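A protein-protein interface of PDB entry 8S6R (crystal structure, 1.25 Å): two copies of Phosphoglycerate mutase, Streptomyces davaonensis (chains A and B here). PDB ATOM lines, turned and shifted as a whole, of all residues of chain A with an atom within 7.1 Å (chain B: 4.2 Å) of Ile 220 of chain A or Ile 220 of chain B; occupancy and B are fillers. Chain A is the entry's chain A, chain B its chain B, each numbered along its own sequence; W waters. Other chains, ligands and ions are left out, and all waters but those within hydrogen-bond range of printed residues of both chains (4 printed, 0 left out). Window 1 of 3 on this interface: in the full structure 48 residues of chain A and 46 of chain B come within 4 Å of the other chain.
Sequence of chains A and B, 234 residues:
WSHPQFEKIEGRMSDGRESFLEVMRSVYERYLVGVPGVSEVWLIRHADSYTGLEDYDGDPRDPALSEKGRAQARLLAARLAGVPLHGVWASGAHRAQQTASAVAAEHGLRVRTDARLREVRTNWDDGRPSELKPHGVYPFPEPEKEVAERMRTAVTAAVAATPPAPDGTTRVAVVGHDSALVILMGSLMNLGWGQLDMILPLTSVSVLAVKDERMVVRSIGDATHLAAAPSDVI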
ATOM      1  N   VAL A 182     -29.544 -12.526 -29.835  1.00  0.00           N
ATOM      2  CA  VAL A 182     -29.381 -13.860 -29.243  1.00  0.00           C
ATOM      3  C   VAL A 182     -30.197 -14.904 -30.007  1.00  0.00           C
ATOM      4  O   VAL A 182     -29.747 -16.048 -30.198  1.00  0.00           O
ATOM      5  CB  VAL A 182     -29.733 -13.842 -27.731  1.00  0.00           C
ATOM      6  CG1 VAL A 182     -29.839 -15.260 -27.166  1.00  0.00           C
ATOM      7  CG2 VAL A 182     -28.705 -13.022 -26.940  1.00  0.00           C
ATOM      8  N   MET A 185     -28.279 -15.655 -33.240  1.00  0.00           N
ATOM      9  CA  MET A 185     -27.090 -16.489 -33.107  1.00  0.00           C
ATOM     10  C   MET A 185     -27.438 -17.890 -32.645  1.00  0.00           C
ATOM     11  O   MET A 185     -26.872 -18.866 -33.168  1.00  0.00           O
ATOM     12  CB  MET A 185     -26.094 -15.835 -32.157  1.00  0.00           C
ATOM     13  CG  MET A 185     -25.383 -14.620 -32.812  1.00  0.00           C
ATOM     14  SD  MET A 185     -24.165 -13.820 -31.775  1.00  0.00           S
ATOM     15  CE  MET A 185     -25.234 -12.891 -30.666  1.00  0.00           C
ATOM     16  N   GLY A 186     -28.416 -18.042 -31.749  1.00  0.00           N
ATOM     17  CA  GLY A 186     -28.896 -19.381 -31.427  1.00  0.00           C
ATOM     18  C   GLY A 186     -29.419 -20.124 -32.642  1.00  0.00           C
ATOM     19  O   GLY A 186     -29.046 -21.265 -32.882  1.00  0.00           O
ATOM     20  N   MET A 189     -27.018 -21.747 -34.907  1.00  0.00           N
ATOM     21  CA  MET A 189     -26.482 -22.987 -34.377  1.00  0.00           C
ATOM     22  C   MET A 189     -27.559 -24.032 -34.169  1.00  0.00           C
ATOM     23  O   MET A 189     -27.319 -25.033 -33.489  1.00  0.00           O
ATOM     24  CB  MET A 189     -25.743 -22.720 -33.071  1.00  0.00           C
ATOM     25  CG  MET A 189     -24.353 -22.146 -33.320  1.00  0.00           C
ATOM     26  SD  MET A 189     -23.453 -21.858 -31.784  1.00  0.00           S
ATOM     27  CE  MET A 189     -24.380 -20.569 -31.048  1.00  0.00           C
ATOM     28  N   LEU A 196     -28.535 -21.280 -25.892  1.00  0.00           N
ATOM     29  CA  LEU A 196     -27.491 -20.254 -25.834  1.00  0.00           C
ATOM     30  C   LEU A 196     -27.949 -19.234 -24.807  1.00  0.00           C
ATOM     31  O   LEU A 196     -28.663 -18.278 -25.103  1.00  0.00           O
ATOM     32  CB  LEU A 196     -27.311 -19.612 -27.199  1.00  0.00           C
ATOM     33  CG  LEU A 196     -26.166 -18.609 -27.249  1.00  0.00           C
ATOM     34  CD1 LEU A 196     -24.803 -19.316 -27.103  1.00  0.00           C
ATOM     35  CD2 LEU A 196     -26.234 -17.836 -28.593  1.00  0.00           C
ATOM     36  N   MET A 198     -27.619 -16.529 -22.672  1.00  0.00           N
ATOM     37  CA  MET A 198     -26.757 -15.363 -22.500  1.00  0.00           C
ATOM     38  C   MET A 198     -27.584 -14.091 -22.674  1.00  0.00           C
ATOM     39  O   MET A 198     -28.531 -14.055 -23.481  1.00  0.00           O
ATOM     40  CB  MET A 198     -25.690 -15.366 -23.609  1.00  0.00           C
ATOM     41  CG  MET A 198     -24.705 -16.490 -23.477  1.00  0.00           C
ATOM     42  SD  MET A 198     -23.479 -16.629 -24.832  1.00  0.00           S
ATOM     43  CE  MET A 198     -22.375 -15.326 -24.326  1.00  0.00           C
ATOM     44  N   LEU A 200     -26.629 -10.350 -23.885  1.00  0.00           N
ATOM     45  CA  LEU A 200     -25.517  -9.659 -24.518  1.00  0.00           C
ATOM     46  C   LEU A 200     -25.279  -8.327 -23.807  1.00  0.00           C
ATOM     47  O   LEU A 200     -26.229  -7.527 -23.634  1.00  0.00           O
ATOM     48  CB  LEU A 200     -25.785  -9.404 -25.994  1.00  0.00           C
ATOM     49  CG  LEU A 200     -26.031 -10.659 -26.802  1.00  0.00           C
ATOM     50  CD1 LEU A 200     -26.381 -10.282 -28.217  1.00  0.00           C
ATOM     51  CD2 LEU A 200     -24.800 -11.593 -26.805  1.00  0.00           C
ATOM     52  N   PRO A 201     -24.045  -8.016 -23.393  1.00  0.00           N
ATOM     53  CA  PRO A 201     -23.798  -6.719 -22.742  1.00  0.00           C
ATOM     54  C   PRO A 201     -24.102  -5.550 -23.663  1.00  0.00           C
ATOM     55  O   PRO A 201     -24.012  -5.648 -24.889  1.00  0.00           O
ATOM     56  CB  PRO A 201     -22.302  -6.768 -22.426  1.00  0.00           C
ATOM     57  CG  PRO A 201     -22.031  -8.251 -22.235  1.00  0.00           C
ATOM     58  CD  PRO A 201     -22.864  -8.897 -23.327  1.00  0.00           C
ATOM     59  N   SER A 204     -21.862  -4.650 -26.631  1.00  0.00           N
ATOM     60  CA  SER A 204     -21.033  -5.801 -26.936  1.00  0.00           C
ATOM     61  C   SER A 204     -20.952  -6.038 -28.439  1.00  0.00           C
ATOM     62  O   SER A 204     -21.854  -5.678 -29.197  1.00  0.00           O
ATOM     63  CB  SER A 204     -21.577  -7.063 -26.285  1.00  0.00           C
ATOM     64  OG  SER A 204     -22.876  -7.402 -26.733  1.00  0.00           O
ATOM     65  N   VAL A 205     -19.872  -6.693 -28.837  1.00  0.00           N
ATOM     66  CA  VAL A 205     -19.568  -7.071 -30.207  1.00  0.00           C
ATOM     67  C   VAL A 205     -19.622  -8.593 -30.298  1.00  0.00           C
ATOM     68  O   VAL A 205     -18.955  -9.307 -29.525  1.00  0.00           O
ATOM     69  CB  VAL A 205     -18.165  -6.604 -30.583  1.00  0.00           C
ATOM     70  CG1 VAL A 205     -17.744  -7.195 -31.945  1.00  0.00           C
ATOM     71  CG2 VAL A 205     -18.055  -5.083 -30.514  1.00  0.00           C
ATOM     72  N   SER A 206     -20.403  -9.095 -31.257  1.00  0.00           N
ATOM     73  CA  SER A 206     -20.423 -10.510 -31.633  1.00  0.00           C
ATOM     74  C   SER A 206     -20.101 -10.560 -33.119  1.00  0.00           C
ATOM     75  O   SER A 206     -20.412  -9.617 -33.845  1.00  0.00           O
ATOM     76  CB  SER A 206     -21.807 -11.094 -31.364  1.00  0.00           C
ATOM     77  OG  SER A 206     -22.263 -10.906 -30.025  1.00  0.00           O
ATOM     78  N   VAL A 207     -19.383 -11.590 -33.563  1.00  0.00           N
ATOM     79  CA  VAL A 207     -18.901 -11.645 -34.941  1.00  0.00           C
ATOM     80  C   VAL A 207     -19.518 -12.847 -35.656  1.00  0.00           C
ATOM     81  O   VAL A 207     -19.525 -13.968 -35.114  1.00  0.00           O
ATOM     82  CB  VAL A 207     -17.369 -11.700 -35.027  1.00  0.00           C
ATOM     83  CG1 VAL A 207     -16.917 -11.816 -36.496  1.00  0.00           C
ATOM     84  CG2 VAL A 207     -16.753 -10.471 -34.312  1.00  0.00           C
ATOM     85  N   VAL A 217     -21.369 -18.453 -36.451  1.00  0.00           N
ATOM     86  CA  VAL A 217     -21.175 -17.675 -35.235  1.00  0.00           C
ATOM     87  C   VAL A 217     -19.710 -17.816 -34.799  1.00  0.00           C
ATOM     88  O   VAL A 217     -19.280 -18.888 -34.361  1.00  0.00           O
ATOM     89  CB  VAL A 217     -22.137 -18.115 -34.134  1.00  0.00           C
ATOM     90  CG1 VAL A 217     -21.890 -17.264 -32.878  1.00  0.00           C
ATOM     91  CG2 VAL A 217     -23.563 -17.978 -34.628  1.00  0.00           C
ATOM     92  N   ARG A 218     -18.930 -16.740 -34.908  1.00  0.00           N
ATOM     93  CA  ARG A 218     -17.500 -16.744 -34.584  1.00  0.00           C
ATOM     94  C   ARG A 218     -17.226 -16.329 -33.137  1.00  0.00           C
ATOM     95  O   ARG A 218     -16.374 -16.925 -32.454  1.00  0.00           O
ATOM     96  CB  ARG A 218     -16.785 -15.808 -35.551  1.00  0.00           C
ATOM     97  CG  ARG A 218     -15.365 -15.418 -35.222  1.00  0.00           C
ATOM     98  CD  ARG A 218     -14.320 -16.393 -35.730  1.00  0.00           C
ATOM     99  NE  ARG A 218     -14.414 -16.683 -37.161  1.00  0.00           N
ATOM    100  CZ  ARG A 218     -14.773 -17.845 -37.690  1.00  0.00           C
ATOM    101  NH1 ARG A 218     -15.177 -18.869 -36.940  1.00  0.00           N
ATOM    102  NH2 ARG A 218     -14.709 -17.994 -39.018  1.00  0.00           N
ATOM    103  N   SER A 219     -17.917 -15.289 -32.694  1.00  0.00           N
ATOM    104  CA  SER A 219     -17.691 -14.845 -31.314  1.00  0.00           C
ATOM    105  C   SER A 219     -18.945 -14.151 -30.813  1.00  0.00           C
ATOM    106  O   SER A 219     -19.776 -13.674 -31.605  1.00  0.00           O
ATOM    107  CB  SER A 219     -16.480 -13.916 -31.200  1.00  0.00           C
ATOM    108  OG  SER A 219     -16.584 -12.774 -32.014  1.00  0.00           O
ATOM    109  N   ILE A 220     -19.120 -14.118 -29.487  1.00  0.00           N
ATOM    110  CA  ILE A 220     -20.390 -13.668 -28.921  1.00  0.00           C
ATOM    111  C   ILE A 220     -20.148 -12.747 -27.723  1.00  0.00           C
ATOM    112  O   ILE A 220     -19.478 -13.151 -26.769  1.00  0.00           O
ATOM    113  CB  ILE A 220     -21.228 -14.844 -28.418  1.00  0.00           C
ATOM    114  CG1 ILE A 220     -21.459 -15.890 -29.543  1.00  0.00           C
ATOM    115  CG2 ILE A 220     -22.562 -14.313 -27.928  1.00  0.00           C
ATOM    116  CD1 ILE A 220     -22.135 -17.166 -29.100  1.00  0.00           C
ATOM    117  N   GLY A 221     -20.785 -11.567 -27.704  1.00  0.00           N
ATOM    118  CA  GLY A 221     -20.992 -10.856 -26.442  1.00  0.00           C
ATOM    119  C   GLY A 221     -19.835 -10.057 -25.861  1.00  0.00           C
ATOM    120  O   GLY A 221     -19.912  -9.741 -24.675  1.00  0.00           O
ATOM    121  N   ASP A 222     -18.838  -9.710 -26.630  1.00  0.00           N
ATOM    122  CA  ASP A 222     -17.629  -9.102 -26.043  1.00  0.00           C
ATOM    123  C   ASP A 222     -17.822  -7.587 -25.829  1.00  0.00           C
ATOM    124  O   ASP A 222     -17.928  -6.827 -26.792  1.00  0.00           O
ATOM    125  CB  ASP A 222     -16.433  -9.407 -26.945  1.00  0.00           C
ATOM    126  CG  ASP A 222     -15.131  -8.864 -26.396  1.00  0.00           C
ATOM    127  OD1 ASP A 222     -15.034  -7.621 -26.202  1.00  0.00           O
ATOM    128  OD2 ASP A 222     -14.210  -9.657 -26.122  1.00  0.00           O
ATOM    129  N   ALA A 223     -17.758  -7.157 -24.559  1.00  0.00           N
ATOM    130  CA  ALA A 223     -17.805  -5.739 -24.201  1.00  0.00           C
ATOM    131  C   ALA A 223     -16.541  -5.342 -23.437  1.00  0.00           C
ATOM    132  O   ALA A 223     -16.572  -4.535 -22.494  1.00  0.00           O
ATOM    133  CB  ALA A 223     -19.087  -5.374 -23.439  1.00  0.00           C
ATOM    134  N   MET B 185     -17.121 -24.098 -21.388  1.00  0.00           N
ATOM    135  CA  MET B 185     -18.169 -23.093 -21.561  1.00  0.00           C
ATOM    136  C   MET B 185     -19.510 -23.753 -21.871  1.00  0.00           C
ATOM    137  O   MET B 185     -20.549 -23.311 -21.354  1.00  0.00           O
ATOM    138  CB  MET B 185     -17.779 -22.065 -22.578  1.00  0.00           C
ATOM    139  CG  MET B 185     -16.755 -21.077 -21.992  1.00  0.00           C
ATOM    140  SD  MET B 185     -16.279 -19.742 -23.099  1.00  0.00           S
ATOM    141  CE  MET B 185     -15.141 -20.623 -24.153  1.00  0.00           C
ATOM    142  N   LEU B 196     -22.884 -25.923 -28.443  1.00  0.00           N
ATOM    143  CA  LEU B 196     -22.149 -24.679 -28.604  1.00  0.00           C
ATOM    144  C   LEU B 196     -21.111 -24.962 -29.697  1.00  0.00           C
ATOM    145  O   LEU B 196     -19.985 -25.408 -29.461  1.00  0.00           O
ATOM    146  CB  LEU B 196     -21.454 -24.308 -27.305  1.00  0.00           C
ATOM    147  CG  LEU B 196     -20.792 -22.922 -27.282  1.00  0.00           C
ATOM    148  CD1 LEU B 196     -21.743 -21.748 -27.379  1.00  0.00           C
ATOM    149  CD2 LEU B 196     -19.928 -22.826 -25.980  1.00  0.00           C
ATOM    150  N   MET B 198     -18.702 -24.152 -31.937  1.00  0.00           N
ATOM    151  CA  MET B 198     -17.745 -23.090 -32.233  1.00  0.00           C
ATOM    152  C   MET B 198     -16.314 -23.576 -32.056  1.00  0.00           C
ATOM    153  O   MET B 198     -16.053 -24.411 -31.184  1.00  0.00           O
ATOM    154  CB  MET B 198     -17.949 -21.935 -31.198  1.00  0.00           C
ATOM    155  CG  MET B 198     -19.357 -21.273 -31.293  1.00  0.00           C
ATOM    156  SD  MET B 198     -19.541 -20.037 -30.004  1.00  0.00           S
ATOM    157  CE  MET B 198     -18.446 -18.715 -30.543  1.00  0.00           C
ATOM    158  N   LEU B 200     -12.792 -21.843 -31.047  1.00  0.00           N
ATOM    159  CA  LEU B 200     -12.288 -20.569 -30.491  1.00  0.00           C
ATOM    160  C   LEU B 200     -11.080 -20.108 -31.294  1.00  0.00           C
ATOM    161  O   LEU B 200     -10.151 -20.895 -31.482  1.00  0.00           O
ATOM    162  CB  LEU B 200     -11.898 -20.762 -29.042  1.00  0.00           C
ATOM    163  CG  LEU B 200     -13.047 -21.212 -28.162  1.00  0.00           C
ATOM    164  CD1 LEU B 200     -12.519 -21.368 -26.769  1.00  0.00           C
ATOM    165  CD2 LEU B 200     -14.181 -20.160 -28.191  1.00  0.00           C
ATOM    166  N   VAL B 205     -10.386 -14.225 -26.594  1.00  0.00           N
ATOM    167  CA  VAL B 205     -10.761 -13.953 -25.204  1.00  0.00           C
ATOM    168  C   VAL B 205     -12.231 -14.328 -25.017  1.00  0.00           C
ATOM    169  O   VAL B 205     -13.089 -13.888 -25.801  1.00  0.00           O
ATOM    170  CB  VAL B 205     -10.574 -12.452 -24.907  1.00  0.00           C
ATOM    171  CG1 VAL B 205     -11.104 -12.084 -23.517  1.00  0.00           C
ATOM    172  CG2 VAL B 205      -9.074 -12.072 -25.055  1.00  0.00           C
ATOM    173  N   SER B 206     -12.503 -15.092 -23.981  1.00  0.00           N
ATOM    174  CA  SER B 206     -13.864 -15.394 -23.549  1.00  0.00           C
ATOM    175  C   SER B 206     -13.939 -15.013 -22.085  1.00  0.00           C
ATOM    176  O   SER B 206     -12.933 -15.119 -21.380  1.00  0.00           O
ATOM    177  CB  SER B 206     -14.140 -16.895 -23.704  1.00  0.00           C
ATOM    178  OG  SER B 206     -13.908 -17.338 -25.058  1.00  0.00           O
ATOM    179  N   VAL B 217     -21.258 -17.714 -18.337  1.00  0.00           N
ATOM    180  CA  VAL B 217     -20.523 -17.413 -19.559  1.00  0.00           C
ATOM    181  C   VAL B 217     -21.016 -16.063 -20.071  1.00  0.00           C
ATOM    182  O   VAL B 217     -22.181 -15.951 -20.502  1.00  0.00           O
ATOM    183  CB  VAL B 217     -20.733 -18.512 -20.622  1.00  0.00           C
ATOM    184  CG1 VAL B 217     -19.974 -18.152 -21.861  1.00  0.00           C
ATOM    185  CG2 VAL B 217     -20.241 -19.843 -20.069  1.00  0.00           C
ATOM    186  N   SER B 219     -18.997 -13.911 -22.435  1.00  0.00           N
ATOM    187  CA  SER B 219     -18.619 -13.676 -23.804  1.00  0.00           C
ATOM    188  C   SER B 219     -17.705 -14.795 -24.256  1.00  0.00           C
ATOM    189  O   SER B 219     -17.080 -15.465 -23.433  1.00  0.00           O
ATOM    190  CB  SER B 219     -18.007 -12.297 -24.046  1.00  0.00           C
ATOM    191  OG  SER B 219     -16.796 -12.151 -23.287  1.00  0.00           O
ATOM    192  N   ILE B 220     -17.689 -15.031 -25.574  1.00  0.00           N
ATOM    193  CA  ILE B 220     -17.055 -16.221 -26.125  1.00  0.00           C
ATOM    194  C   ILE B 220     -16.277 -15.877 -27.364  1.00  0.00           C
ATOM    195  O   ILE B 220     -16.838 -15.374 -28.346  1.00  0.00           O
ATOM    196  CB  ILE B 220     -18.087 -17.294 -26.504  1.00  0.00           C
ATOM    197  CG1 ILE B 220     -18.939 -17.678 -25.329  1.00  0.00           C
ATOM    198  CG2 ILE B 220     -17.339 -18.570 -26.996  1.00  0.00           C
ATOM    199  CD1 ILE B 220     -20.101 -18.593 -25.676  1.00  0.00           C
ATOM    200  N   GLY B 221     -14.987 -16.214 -27.380  1.00  0.00           N
ATOM    201  CA  GLY B 221     -14.328 -16.349 -28.669  1.00  0.00           C
ATOM    202  C   GLY B 221     -13.800 -15.132 -29.396  1.00  0.00           C
ATOM    203  O   GLY B 221     -13.522 -15.211 -30.605  1.00  0.00           O
ATOM    204  N   ASP B 222     -13.666 -13.980 -28.721  1.00  0.00           N
ATOM    205  CA  ASP B 222     -13.334 -12.722 -29.403  1.00  0.00           C
ATOM    206  C   ASP B 222     -11.824 -12.637 -29.693  1.00  0.00           C
ATOM    207  O   ASP B 222     -10.999 -12.528 -28.772  1.00  0.00           O
ATOM    208  CB  ASP B 222     -13.811 -11.558 -28.531  1.00  0.00           C
ATOM    209  CG  ASP B 222     -13.602 -10.208 -29.175  1.00  0.00           C
ATOM    210  OD1 ASP B 222     -12.449  -9.836 -29.440  1.00  0.00           O
ATOM    211  OD2 ASP B 222     -14.605  -9.513 -29.403  1.00  0.00           O
HETATM  212  O   HOH W   1     -13.761 -12.649 -32.902  1.00  0.00           O
HETATM  213  O   HOH W   2     -16.789 -10.746 -30.314  1.00  0.00           O
HETATM  214  O   HOH W   3     -14.895 -11.978 -25.048  1.00  0.00           O
HETATM  215  O   HOH W   4     -17.106  -9.328 -22.512  1.00  0.00           O
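Ile 220 of chain A touches three residues of chain B.
Printed residues of chain A within 4 Å of Ile 220 of chain B: Met 198 (3.998 Å), Ser 219 (3.1 Å) and Ile 220 (2.8 Å).
Printed residues of chain A within 4 Å of Leu 196 of chain B: Leu 196 (3.9 Å).
Of the printed residues of chain A, Met 198 of chain B touches Val 217, Arg 218 and Ile 220.
The nearest printed residue of chain B that does not touch Ile 220 of chain A is Leu 196 of chain B (4.9 Å).
The nearest printed residue of chain A that does not touch Ile 220 of chain B is Arg 218 of chain A (4.4 Å).
The backbone NH (N) of Ile 220 of chain A sits at hydrogen-bond distance from the backbone carbonyl oxygen (O) of Ile 220 of chain B (2.8 Å).
The side-chain carboxylate (OD2) of Asp 222 of chain A sits close to the side-chain carboxylate (OD2) of Asp 222 of chain B (3.3 Å).
The backbone carbonyl oxygen (O) of Val 207 of chain A is in hydrogen-bond range of the backbone NH (N) of Arg 218 of chain A, 2.8 Å away.
The backbone NH (N) of Val 205 of chain B sits at hydrogen-bond distance from the backbone carbonyl oxygen (O) of Asp 222 of chain B.
The backbone NH (N) of Val 207 of chain A sits at hydrogen-bond distance from the backbone carbonyl oxygen (O) of Ser 219 of chain A (2.9 Å).
OG of Ser 206 of chain B is in hydrogen-bond range of N of Gly 221 of chain B.
The backbone carbonyl oxygen (O) of Val 205 of chain B is in hydrogen-bond range of the backbone NH (N) of Gly 221 of chain B, at 3.4 Å.
The backbone NH of Gly 221 of chain A sits at hydrogen-bond distance from the side-chain hydroxyl of Ser 206 of chain A, at 2.8 Å.
Ser 219 of chain A touches Ile 220 of chain B, and with the chains exchanged Ile 220 of chain A touches Ser 219 of chain B.
Ser 219 of chain A touches Gly 221 of chain B, and with the chains exchanged Gly 221 of chain A touches Ser 219 of chain B.
Ile 220 of chain B touches its own counterpart, Ile 220 of chain A.
Asp 222 of chain B touches its own counterpart, Asp 222 of chain A.
Of the 15 pairs that touch across the chains among the printed residues, 13 have their exchanged pair printed and touching as well.
Leu 196 of chain B touches Leu 196 of chain A.
Met 198 of chain A touches Val 217 of chain B.
Val 217 of chain A touches Met 198 of chain B.
O of Arg 218 of chain A touches CE of Met 198 of chain B, 3.3 Å away.
Gly 221 of chain B touches Arg 218 of chain A.
Ser 219 of chain A touches Gly 221 of chain B (CB to O, 3.3 Å).
CB of Ser 219 of chain A touches N of Asp 222 of chain B, at 3.8 Å.
Met 198 of chain B touches Ile 220 of chain A.
Ile 220 of chain A touches Ser 219 of chain B.
Ser 219 of chain B touches Asp 222 of chain A.
Printed residues of chain A that touch a printed residue of chain B: Leu 196, Met 198, Val 217, Arg 218, Ser 219, Ile 220, Gly 221 and Asp 222.
Hydrophobic or aromatic side chains of chain A that line the printed part of chain B: Leu 196, Met 198 and Ile 220.
Hydrophobic or aromatic side chains of chain B that line the printed part of chain A: Leu 196, Met 198 and Ile 220.
Among the printed residues, 15 pairs touch across the chains.
Among the printed residues, no Asp or Glu carboxylate lies within 4 Å of a Lys or Arg side-chain nitrogen of the other chain.
Water W3 lies within hydrogen-bond range of the side-chain hydroxyl (OG) of Ser 219 of chain B (2.6 Å), the side-chain carboxylate (OD2) of Asp 222 of chain A (2.6 Å) and the backbone carbonyl oxygen (O) of Val 205 of chain B (2.7 Å).
Water W2 lies within hydrogen-bond range of OG of Ser 219 of chain A (2.7 Å), OD2 of Asp 222 of chain B (2.7 Å) and O of Val 205 of chain A (2.7 Å).
Water W4 bridges the side-chain hydroxyl (OG) of Ser 219 of chain B and the backbone NH (N) of Ala 223 of chain A.
Water W1 bridges the side-chain hydroxyl of Ser 219 of chain A (3.0 Å) and the backbone carbonyl oxygen of Gly 221 of chain B (3.4 Å).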
